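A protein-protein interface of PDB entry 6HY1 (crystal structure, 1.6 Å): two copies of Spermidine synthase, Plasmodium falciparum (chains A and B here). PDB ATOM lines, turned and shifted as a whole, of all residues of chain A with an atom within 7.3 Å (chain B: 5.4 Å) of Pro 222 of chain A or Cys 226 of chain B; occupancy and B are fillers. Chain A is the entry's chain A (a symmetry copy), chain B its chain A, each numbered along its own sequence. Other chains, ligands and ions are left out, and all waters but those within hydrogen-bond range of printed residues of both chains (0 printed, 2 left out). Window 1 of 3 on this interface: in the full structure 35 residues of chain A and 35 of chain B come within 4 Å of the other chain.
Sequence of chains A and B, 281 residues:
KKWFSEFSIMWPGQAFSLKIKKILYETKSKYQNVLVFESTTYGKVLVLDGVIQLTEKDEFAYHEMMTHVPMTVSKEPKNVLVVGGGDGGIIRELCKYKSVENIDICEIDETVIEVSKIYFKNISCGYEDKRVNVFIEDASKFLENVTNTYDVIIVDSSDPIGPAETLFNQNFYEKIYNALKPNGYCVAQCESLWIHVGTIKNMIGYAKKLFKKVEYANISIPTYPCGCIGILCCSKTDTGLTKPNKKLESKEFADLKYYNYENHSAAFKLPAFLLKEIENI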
ATOM      1  N   PHE A  16      -3.544  -3.405  10.258  1.00  0.00           N
ATOM      2  CA  PHE A  16      -4.688  -2.909   9.517  1.00  0.00           C
ATOM      3  C   PHE A  16      -5.135  -1.641  10.222  1.00  0.00           C
ATOM      4  O   PHE A  16      -5.072  -1.582  11.446  1.00  0.00           O
ATOM      5  CB  PHE A  16      -5.833  -3.972   9.502  1.00  0.00           C
ATOM      6  CG  PHE A  16      -7.086  -3.515   8.853  1.00  0.00           C
ATOM      7  CD1 PHE A  16      -7.144  -3.290   7.499  1.00  0.00           C
ATOM      8  CD2 PHE A  16      -8.242  -3.309   9.613  1.00  0.00           C
ATOM      9  CE1 PHE A  16      -8.307  -2.881   6.895  1.00  0.00           C
ATOM     10  CE2 PHE A  16      -9.428  -2.903   9.015  1.00  0.00           C
ATOM     11  CZ  PHE A  16      -9.474  -2.678   7.670  1.00  0.00           C
ATOM     12  N   TYR A  42     -16.478   1.893   8.015  1.00  0.00           N
ATOM     13  CA  TYR A  42     -16.928   0.610   8.545  1.00  0.00           C
ATOM     14  C   TYR A  42     -17.949   0.754   9.681  1.00  0.00           C
ATOM     15  O   TYR A  42     -18.258  -0.239  10.362  1.00  0.00           O
ATOM     16  CB  TYR A  42     -15.725  -0.222   9.004  1.00  0.00           C
ATOM     17  CG  TYR A  42     -15.033  -0.918   7.842  1.00  0.00           C
ATOM     18  CD1 TYR A  42     -14.226  -0.204   6.975  1.00  0.00           C
ATOM     19  CD2 TYR A  42     -15.247  -2.264   7.596  1.00  0.00           C
ATOM     20  CE1 TYR A  42     -13.589  -0.837   5.895  1.00  0.00           C
ATOM     21  CE2 TYR A  42     -14.627  -2.906   6.510  1.00  0.00           C
ATOM     22  CZ  TYR A  42     -13.805  -2.163   5.684  1.00  0.00           C
ATOM     23  OH  TYR A  42     -13.198  -2.774   4.616  1.00  0.00           O
ATOM     24  N   ILE A  52      -9.322  -5.291  17.186  1.00  0.00           N
ATOM     25  CA  ILE A  52     -10.685  -5.069  16.705  1.00  0.00           C
ATOM     26  C   ILE A  52     -11.520  -6.301  17.020  1.00  0.00           C
ATOM     27  O   ILE A  52     -11.185  -7.423  16.614  1.00  0.00           O
ATOM     28  CB  ILE A  52     -10.695  -4.751  15.198  1.00  0.00           C
ATOM     29  CG1 ILE A  52      -9.918  -3.447  14.925  1.00  0.00           C
ATOM     30  CG2 ILE A  52     -12.142  -4.721  14.653  1.00  0.00           C
ATOM     31  CD1 ILE A  52      -9.629  -3.209  13.427  1.00  0.00           C
ATOM     32  N   THR A  55     -16.906  -4.661  13.710  1.00  0.00           N
ATOM     33  CA  THR A  55     -17.381  -3.421  13.125  1.00  0.00           C
ATOM     34  C   THR A  55     -18.791  -3.635  12.600  1.00  0.00           C
ATOM     35  O   THR A  55     -19.181  -4.760  12.252  1.00  0.00           O
ATOM     36  CB  THR A  55     -16.484  -2.885  11.972  1.00  0.00           C
ATOM     37  OG1 THR A  55     -16.820  -3.580  10.770  1.00  0.00           O
ATOM     38  CG2 THR A  55     -14.984  -3.018  12.257  1.00  0.00           C
ATOM     39  N   LYS A  57     -20.000  -2.879   9.810  1.00  0.00           N
ATOM     40  CA  LYS A  57     -20.096  -3.181   8.380  1.00  0.00           C
ATOM     41  C   LYS A  57     -19.992  -4.676   8.115  1.00  0.00           C
ATOM     42  O   LYS A  57     -20.640  -5.188   7.191  1.00  0.00           O
ATOM     43  CB  LYS A  57     -19.017  -2.425   7.600  1.00  0.00           C
ATOM     44  CG  LYS A  57     -18.893  -2.836   6.095  1.00  0.00           C
ATOM     45  CD  LYS A  57     -18.023  -1.808   5.316  1.00  0.00           C
ATOM     46  CE  LYS A  57     -17.746  -2.238   3.853  1.00  0.00           C
ATOM     47  NZ  LYS A  57     -19.017  -2.273   3.088  1.00  0.00           N
ATOM     48  N   ASP A  58     -19.165  -5.400   8.880  1.00  0.00           N
ATOM     49  CA  ASP A  58     -18.929  -6.785   8.516  1.00  0.00           C
ATOM     50  C   ASP A  58     -19.217  -7.813   9.607  1.00  0.00           C
ATOM     51  O   ASP A  58     -19.019  -9.008   9.370  1.00  0.00           O
ATOM     52  CB  ASP A  58     -17.477  -6.950   8.014  1.00  0.00           C
ATOM     53  CG  ASP A  58     -16.444  -6.639   9.071  1.00  0.00           C
ATOM     54  OD1 ASP A  58     -16.830  -6.238  10.198  1.00  0.00           O
ATOM     55  OD2 ASP A  58     -15.222  -6.754   8.790  1.00  0.00           O
ATOM     56  N   GLU A  59     -19.734  -7.409  10.776  1.00  0.00           N
ATOM     57  CA  GLU A  59     -19.837  -8.380  11.865  1.00  0.00           C
ATOM     58  C   GLU A  59     -20.792  -9.518  11.529  1.00  0.00           C
ATOM     59  O   GLU A  59     -20.649 -10.609  12.073  1.00  0.00           O
ATOM     60  CB  GLU A  59     -20.295  -7.688  13.165  1.00  0.00           C
ATOM     61  CG  GLU A  59     -21.572  -6.872  13.022  1.00  0.00           C
ATOM     62  CD  GLU A  59     -22.876  -7.693  13.164  1.00  0.00           C
ATOM     63  OE1 GLU A  59     -22.854  -8.888  13.569  1.00  0.00           O
ATOM     64  OE2 GLU A  59     -23.921  -7.110  12.847  1.00  0.00           O
ATOM     65  N   ALA A  61     -20.884 -11.418   9.078  1.00  0.00           N
ATOM     66  CA  ALA A  61     -20.237 -12.580   8.481  1.00  0.00           C
ATOM     67  C   ALA A  61     -19.808 -13.549   9.566  1.00  0.00           C
ATOM     68  O   ALA A  61     -20.091 -14.750   9.500  1.00  0.00           O
ATOM     69  CB  ALA A  61     -19.025 -12.142   7.638  1.00  0.00           C
ATOM     70  N   ILE A 219     -13.897 -18.248   7.534  1.00  0.00           N
ATOM     71  CA  ILE A 219     -14.847 -17.153   7.337  1.00  0.00           C
ATOM     72  C   ILE A 219     -14.087 -15.969   6.745  1.00  0.00           C
ATOM     73  O   ILE A 219     -13.046 -15.588   7.269  1.00  0.00           O
ATOM     74  CB  ILE A 219     -15.508 -16.690   8.662  1.00  0.00           C
ATOM     75  CG1 ILE A 219     -16.106 -17.878   9.429  1.00  0.00           C
ATOM     76  CG2 ILE A 219     -16.592 -15.642   8.359  1.00  0.00           C
ATOM     77  CD1 ILE A 219     -16.631 -17.465  10.820  1.00  0.00           C
ATOM     78  N   SER A 220     -14.639 -15.358   5.693  1.00  0.00           N
ATOM     79  CA  SER A 220     -14.063 -14.124   5.167  1.00  0.00           C
ATOM     80  C   SER A 220     -14.618 -12.969   5.988  1.00  0.00           C
ATOM     81  O   SER A 220     -15.840 -12.786   6.056  1.00  0.00           O
ATOM     82  CB  SER A 220     -14.409 -13.955   3.681  1.00  0.00           C
ATOM     83  OG  SER A 220     -14.157 -12.633   3.213  1.00  0.00           O
ATOM     84  N   ILE A 221     -13.726 -12.184   6.583  1.00  0.00           N
ATOM     85  CA  ILE A 221     -14.139 -10.988   7.317  1.00  0.00           C
ATOM     86  C   ILE A 221     -12.981  -9.989   7.272  1.00  0.00           C
ATOM     87  O   ILE A 221     -11.914 -10.236   7.853  1.00  0.00           O
ATOM     88  CB  ILE A 221     -14.601 -11.346   8.742  1.00  0.00           C
ATOM     89  CG1 ILE A 221     -14.812 -10.076   9.586  1.00  0.00           C
ATOM     90  CG2 ILE A 221     -13.689 -12.337   9.414  1.00  0.00           C
ATOM     91  CD1 ILE A 221     -15.734 -10.297  10.811  1.00  0.00           C
ATOM     92  N   PRO A 222     -13.177  -8.826   6.646  1.00  0.00           N
ATOM     93  CA  PRO A 222     -12.028  -7.967   6.333  1.00  0.00           C
ATOM     94  C   PRO A 222     -11.376  -7.304   7.533  1.00  0.00           C
ATOM     95  O   PRO A 222     -10.196  -6.934   7.431  1.00  0.00           O
ATOM     96  CB  PRO A 222     -12.622  -6.927   5.370  1.00  0.00           C
ATOM     97  CG  PRO A 222     -14.144  -6.955   5.675  1.00  0.00           C
ATOM     98  CD  PRO A 222     -14.394  -8.397   5.939  1.00  0.00           C
ATOM     99  N   THR A 223     -12.069  -7.124   8.665  1.00  0.00           N
ATOM    100  CA  THR A 223     -11.487  -6.376   9.771  1.00  0.00           C
ATOM    101  C   THR A 223     -10.915  -7.281  10.846  1.00  0.00           C
ATOM    102  O   THR A 223     -10.642  -6.807  11.954  1.00  0.00           O
ATOM    103  CB  THR A 223     -12.517  -5.410  10.377  1.00  0.00           C
ATOM    104  OG1 THR A 223     -13.667  -6.141  10.809  1.00  0.00           O
ATOM    105  CG2 THR A 223     -12.975  -4.374   9.348  1.00  0.00           C
ATOM    106  N   TYR A 224     -10.769  -8.596  10.556  1.00  0.00           N
ATOM    107  CA  TYR A 224      -9.888  -9.400  11.391  1.00  0.00           C
ATOM    108  C   TYR A 224      -8.560  -9.598  10.662  1.00  0.00           C
ATOM    109  O   TYR A 224      -8.524  -9.538   9.425  1.00  0.00           O
ATOM    110  CB  TYR A 224     -10.495 -10.761  11.719  1.00  0.00           C
ATOM    111  CG  TYR A 224     -11.673 -10.728  12.699  1.00  0.00           C
ATOM    112  CD1 TYR A 224     -11.854  -9.680  13.592  1.00  0.00           C
ATOM    113  CD2 TYR A 224     -12.587 -11.768  12.719  1.00  0.00           C
ATOM    114  CE1 TYR A 224     -12.951  -9.672  14.493  1.00  0.00           C
ATOM    115  CE2 TYR A 224     -13.664 -11.758  13.611  1.00  0.00           C
ATOM    116  CZ  TYR A 224     -13.836 -10.725  14.480  1.00  0.00           C
ATOM    117  OH  TYR A 224     -14.934 -10.756  15.348  1.00  0.00           O
ATOM    118  N   PRO A 225      -7.462  -9.820  11.379  1.00  0.00           N
ATOM    119  CA  PRO A 225      -6.144  -9.840  10.711  1.00  0.00           C
ATOM    120  C   PRO A 225      -6.083 -10.937   9.653  1.00  0.00           C
ATOM    121  O   PRO A 225      -6.546 -12.067   9.867  1.00  0.00           O
ATOM    122  CB  PRO A 225      -5.160 -10.133  11.843  1.00  0.00           C
ATOM    123  CG  PRO A 225      -5.923  -9.872  13.146  1.00  0.00           C
ATOM    124  CD  PRO A 225      -7.370  -9.963  12.843  1.00  0.00           C
ATOM    125  N   CYS A 226      -5.473 -10.589   8.512  1.00  0.00           N
ATOM    126  CA  CYS A 226      -5.396 -11.418   7.307  1.00  0.00           C
ATOM    127  C   CYS A 226      -6.744 -11.610   6.608  1.00  0.00           C
ATOM    128  O   CYS A 226      -6.833 -12.366   5.611  1.00  0.00           O
ATOM    129  CB  CYS A 226      -4.743 -12.777   7.605  1.00  0.00           C
ATOM    130  SG  CYS A 226      -2.999 -12.614   8.080  1.00  0.00           S
ATOM    131  N   GLY A 227      -7.810 -10.950   7.080  1.00  0.00           N
ATOM    132  CA  GLY A 227      -9.069 -10.964   6.364  1.00  0.00           C
ATOM    133  C   GLY A 227      -9.897 -12.207   6.561  1.00  0.00           C
ATOM    134  O   GLY A 227     -10.851 -12.407   5.820  1.00  0.00           O
ATOM    135  N   CYS A 228      -9.544 -13.062   7.505  1.00  0.00           N
ATOM    136  CA  CYS A 228     -10.335 -14.266   7.714  1.00  0.00           C
ATOM    137  C   CYS A 228     -10.106 -14.773   9.131  1.00  0.00           C
ATOM    138  O   CYS A 228      -9.168 -14.378   9.811  1.00  0.00           O
ATOM    139  CB  CYS A 228      -9.994 -15.350   6.678  1.00  0.00           C
ATOM    140  SG  CYS A 228      -8.265 -15.897   6.693  1.00  0.00           S
ATOM    141  N   GLN B  14      -9.535   2.858   4.969  1.00  0.00           N
ATOM    142  CA  GLN B  14      -8.884   1.679   5.507  1.00  0.00           C
ATOM    143  C   GLN B  14      -7.487   1.630   4.917  1.00  0.00           C
ATOM    144  O   GLN B  14      -7.230   2.225   3.873  1.00  0.00           O
ATOM    145  CB  GLN B  14      -9.640   0.383   5.146  1.00  0.00           C
ATOM    146  CG  GLN B  14      -9.528   0.041   3.675  1.00  0.00           C
ATOM    147  CD  GLN B  14     -10.398  -1.129   3.286  1.00  0.00           C
ATOM    148  OE1 GLN B  14     -11.636  -1.000   3.247  1.00  0.00           O
ATOM    149  NE2 GLN B  14      -9.770  -2.277   2.983  1.00  0.00           N
ATOM    150  N   SER B 192     -12.987  -6.757  -4.970  1.00  0.00           N
ATOM    151  CA  SER B 192     -13.307  -7.468  -3.728  1.00  0.00           C
ATOM    152  C   SER B 192     -14.767  -7.257  -3.344  1.00  0.00           C
ATOM    153  O   SER B 192     -15.290  -6.141  -3.414  1.00  0.00           O
ATOM    154  CB  SER B 192     -12.420  -6.990  -2.579  1.00  0.00           C
ATOM    155  OG  SER B 192     -12.880  -7.505  -1.325  1.00  0.00           O
ATOM    156  N   TRP B 194     -16.113  -7.163  -0.592  1.00  0.00           N
ATOM    157  CA  TRP B 194     -16.322  -6.294   0.571  1.00  0.00           C
ATOM    158  C   TRP B 194     -16.198  -4.814   0.258  1.00  0.00           C
ATOM    159  O   TRP B 194     -16.471  -3.994   1.140  1.00  0.00           O
ATOM    160  CB  TRP B 194     -15.332  -6.616   1.691  1.00  0.00           C
ATOM    161  CG  TRP B 194     -15.635  -7.878   2.347  1.00  0.00           C
ATOM    162  CD1 TRP B 194     -14.979  -9.064   2.223  1.00  0.00           C
ATOM    163  CD2 TRP B 194     -16.723  -8.106   3.259  1.00  0.00           C
ATOM    164  NE1 TRP B 194     -15.569 -10.022   3.021  1.00  0.00           N
ATOM    165  CE2 TRP B 194     -16.648  -9.456   3.664  1.00  0.00           C
ATOM    166  CE3 TRP B 194     -17.720  -7.277   3.795  1.00  0.00           C
ATOM    167  CZ2 TRP B 194     -17.571 -10.037   4.557  1.00  0.00           C
ATOM    168  CZ3 TRP B 194     -18.662  -7.855   4.699  1.00  0.00           C
ATOM    169  CH2 TRP B 194     -18.555  -9.209   5.081  1.00  0.00           C
ATOM    170  N   ILE B 195     -15.825  -4.437  -0.961  1.00  0.00           N
ATOM    171  CA  ILE B 195     -15.658  -3.018  -1.271  1.00  0.00           C
ATOM    172  C   ILE B 195     -16.719  -2.543  -2.245  1.00  0.00           C
ATOM    173  O   ILE B 195     -17.856  -2.269  -1.842  1.00  0.00           O
ATOM    174  CB  ILE B 195     -14.244  -2.741  -1.813  1.00  0.00           C
ATOM    175  CG1 ILE B 195     -13.228  -3.468  -0.954  1.00  0.00           C
ATOM    176  CG2 ILE B 195     -13.974  -1.266  -1.793  1.00  0.00           C
ATOM    177  CD1 ILE B 195     -11.770  -3.084  -1.283  1.00  0.00           C
ATOM    178  N   TYR B 224      -4.169  -8.409  -0.284  1.00  0.00           N
ATOM    179  CA  TYR B 224      -5.001  -7.525  -1.088  1.00  0.00           C
ATOM    180  C   TYR B 224      -6.063  -6.893  -0.189  1.00  0.00           C
ATOM    181  O   TYR B 224      -6.420  -7.478   0.843  1.00  0.00           O
ATOM    182  CB  TYR B 224      -5.680  -8.265  -2.235  1.00  0.00           C
ATOM    183  CG  TYR B 224      -4.748  -8.699  -3.372  1.00  0.00           C
ATOM    184  CD1 TYR B 224      -3.536  -8.064  -3.608  1.00  0.00           C
ATOM    185  CD2 TYR B 224      -5.111  -9.743  -4.205  1.00  0.00           C
ATOM    186  CE1 TYR B 224      -2.690  -8.480  -4.669  1.00  0.00           C
ATOM    187  CE2 TYR B 224      -4.276 -10.148  -5.251  1.00  0.00           C
ATOM    188  CZ  TYR B 224      -3.088  -9.523  -5.473  1.00  0.00           C
ATOM    189  OH  TYR B 224      -2.283  -9.970  -6.527  1.00  0.00           O
ATOM    190  N   PRO B 225      -6.575  -5.715  -0.533  1.00  0.00           N
ATOM    191  CA  PRO B 225      -7.471  -5.005   0.403  1.00  0.00           C
ATOM    192  C   PRO B 225      -8.713  -5.836   0.710  1.00  0.00           C
ATOM    193  O   PRO B 225      -9.317  -6.447  -0.184  1.00  0.00           O
ATOM    194  CB  PRO B 225      -7.852  -3.728  -0.345  1.00  0.00           C
ATOM    195  CG  PRO B 225      -6.847  -3.594  -1.493  1.00  0.00           C
ATOM    196  CD  PRO B 225      -6.279  -4.937  -1.750  1.00  0.00           C
ATOM    197  N   CYS B 226      -9.101  -5.822   1.992  1.00  0.00           N
ATOM    198  CA  CYS B 226     -10.182  -6.632   2.557  1.00  0.00           C
ATOM    199  C   CYS B 226      -9.870  -8.130   2.597  1.00  0.00           C
ATOM    200  O   CYS B 226     -10.742  -8.945   2.981  1.00  0.00           O
ATOM    201  CB  CYS B 226     -11.511  -6.377   1.829  1.00  0.00           C
ATOM    202  SG  CYS B 226     -12.119  -4.685   2.077  1.00  0.00           S
ATOM    203  N   GLY B 227      -8.650  -8.540   2.223  1.00  0.00           N
ATOM    204  CA  GLY B 227      -8.245  -9.920   2.395  1.00  0.00           C
ATOM    205  C   GLY B 227      -8.759 -10.868   1.343  1.00  0.00           C
ATOM    206  O   GLY B 227      -8.666 -12.073   1.536  1.00  0.00           O
ATOM    207  N   CYS B 228      -9.329 -10.366   0.260  1.00  0.00           N
ATOM    208  CA  CYS B 228      -9.826 -11.267  -0.769  1.00  0.00           C
ATOM    209  C   CYS B 228      -9.907 -10.516  -2.092  1.00  0.00           C
ATOM    210  O   CYS B 228      -9.854  -9.294  -2.140  1.00  0.00           O
ATOM    211  CB  CYS B 228     -11.194 -11.858  -0.388  1.00  0.00           C
ATOM    212  SG  CYS B 228     -12.508 -10.633  -0.138  1.00  0.00           S
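Positions printed for both chains: 224, 225, 226, 227 and 228.
OE1 of Gln 14 of chain B sits at hydrogen-bond distance from OH of Tyr 42 of chain A (2.7 Å).
NE1 of Trp 194 of chain B sits at hydrogen-bond distance from OG of Ser 220 of chain A (3.0 Å).
SG of Cys 226 of chain B lies within hydrogen-bond range of OH of Tyr 42 of chain A, 3.4 Å away.
Printed residues of chain A that touch a printed residue of chain B: Phe 16, Tyr 42, Lys 57, Asp 58, Ala 61, Ser 220 and Pro 222.
Of the 9 printed residues of chain B, 3 touch a printed residue of chain A.
Hydrophobic or aromatic side chains of chain B that line the printed part of chain A: Trp 194.
Among the printed residues, no Asp or Glu carboxylate lies within 4 Å of a Lys or Arg side-chain nitrogen of the other chain.
Printed residues of chain B within 4 Å of Tyr 42 of chain A: Gln 14 (2.7 Å) and Cys 226 (3.4 Å).
Of the printed residues of chain B, Lys 57 of chain A touches Trp 194 (3.5 Å).
Of the printed residues of chain B, Ala 61 of chain A touches Trp 194 (3.9 Å).
Printed residues of chain A within 4 Å of Gln 14 of chain B: Phe 16 and Tyr 42.
Of the printed residues of chain A, Trp 194 of chain B touches Lys 57, Asp 58, Ala 61, Ser 220 and Pro 222.
Ile 195 of chain B touches none of the printed residues of chain A.
Pro 225 of chain B touches none of the printed residues of chain A.
Cys 226 of chain B touches just these residues of chain A: Tyr 42 and Pro 222.
The nearest residue of chain B that does not touch Pro 222 of chain A is Gly 227 of chain B (5.3 Å).
The nearest residue of chain A that does not touch Cys 226 of chain B is Gly 227 of chain A (4.3 Å).
Gln 14 of chain B touches Phe 16 of chain A (CB to CE1, 3.9 Å).
Lys 57 of chain A touches Trp 194 of chain B.
Asp 58 of chain A touches Trp 194 of chain B (CB to CZ3, 3.6 Å).
Ala 61 of chain A touches Trp 194 of chain B (CB to CH2, 3.9 Å).
Pro 222 of chain A touches Trp 194 of chain B.
Pro 222 of chain A touches Cys 226 of chain B.
The side-chain hydroxyl of Ser 192 of chain B lies close to the backbone NH of Trp 194 of chain B (3.3 Å).
OD1 of Asp 58 of chain A is in hydrogen-bond range of OG1 of Thr 55 of chain A, 2.7 Å away.
N of Lys 57 of chain A is in hydrogen-bond range of O of Tyr 42 of chain A, at 3.2 Å.
OD2 of Asp 58 of chain A is in hydrogen-bond range of OG1 of Thr 223 of chain A, at 2.6 Å.
The side-chain hydroxyl (OG1) of Thr 55 of chain A sits close to the backbone NH (N) of Lys 57 of chain A, 3.4 Å away.
SG of Cys 226 of chain B lies within hydrogen-bond range of NE2 of Gln 14 of chain B, at 3.5 Å.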
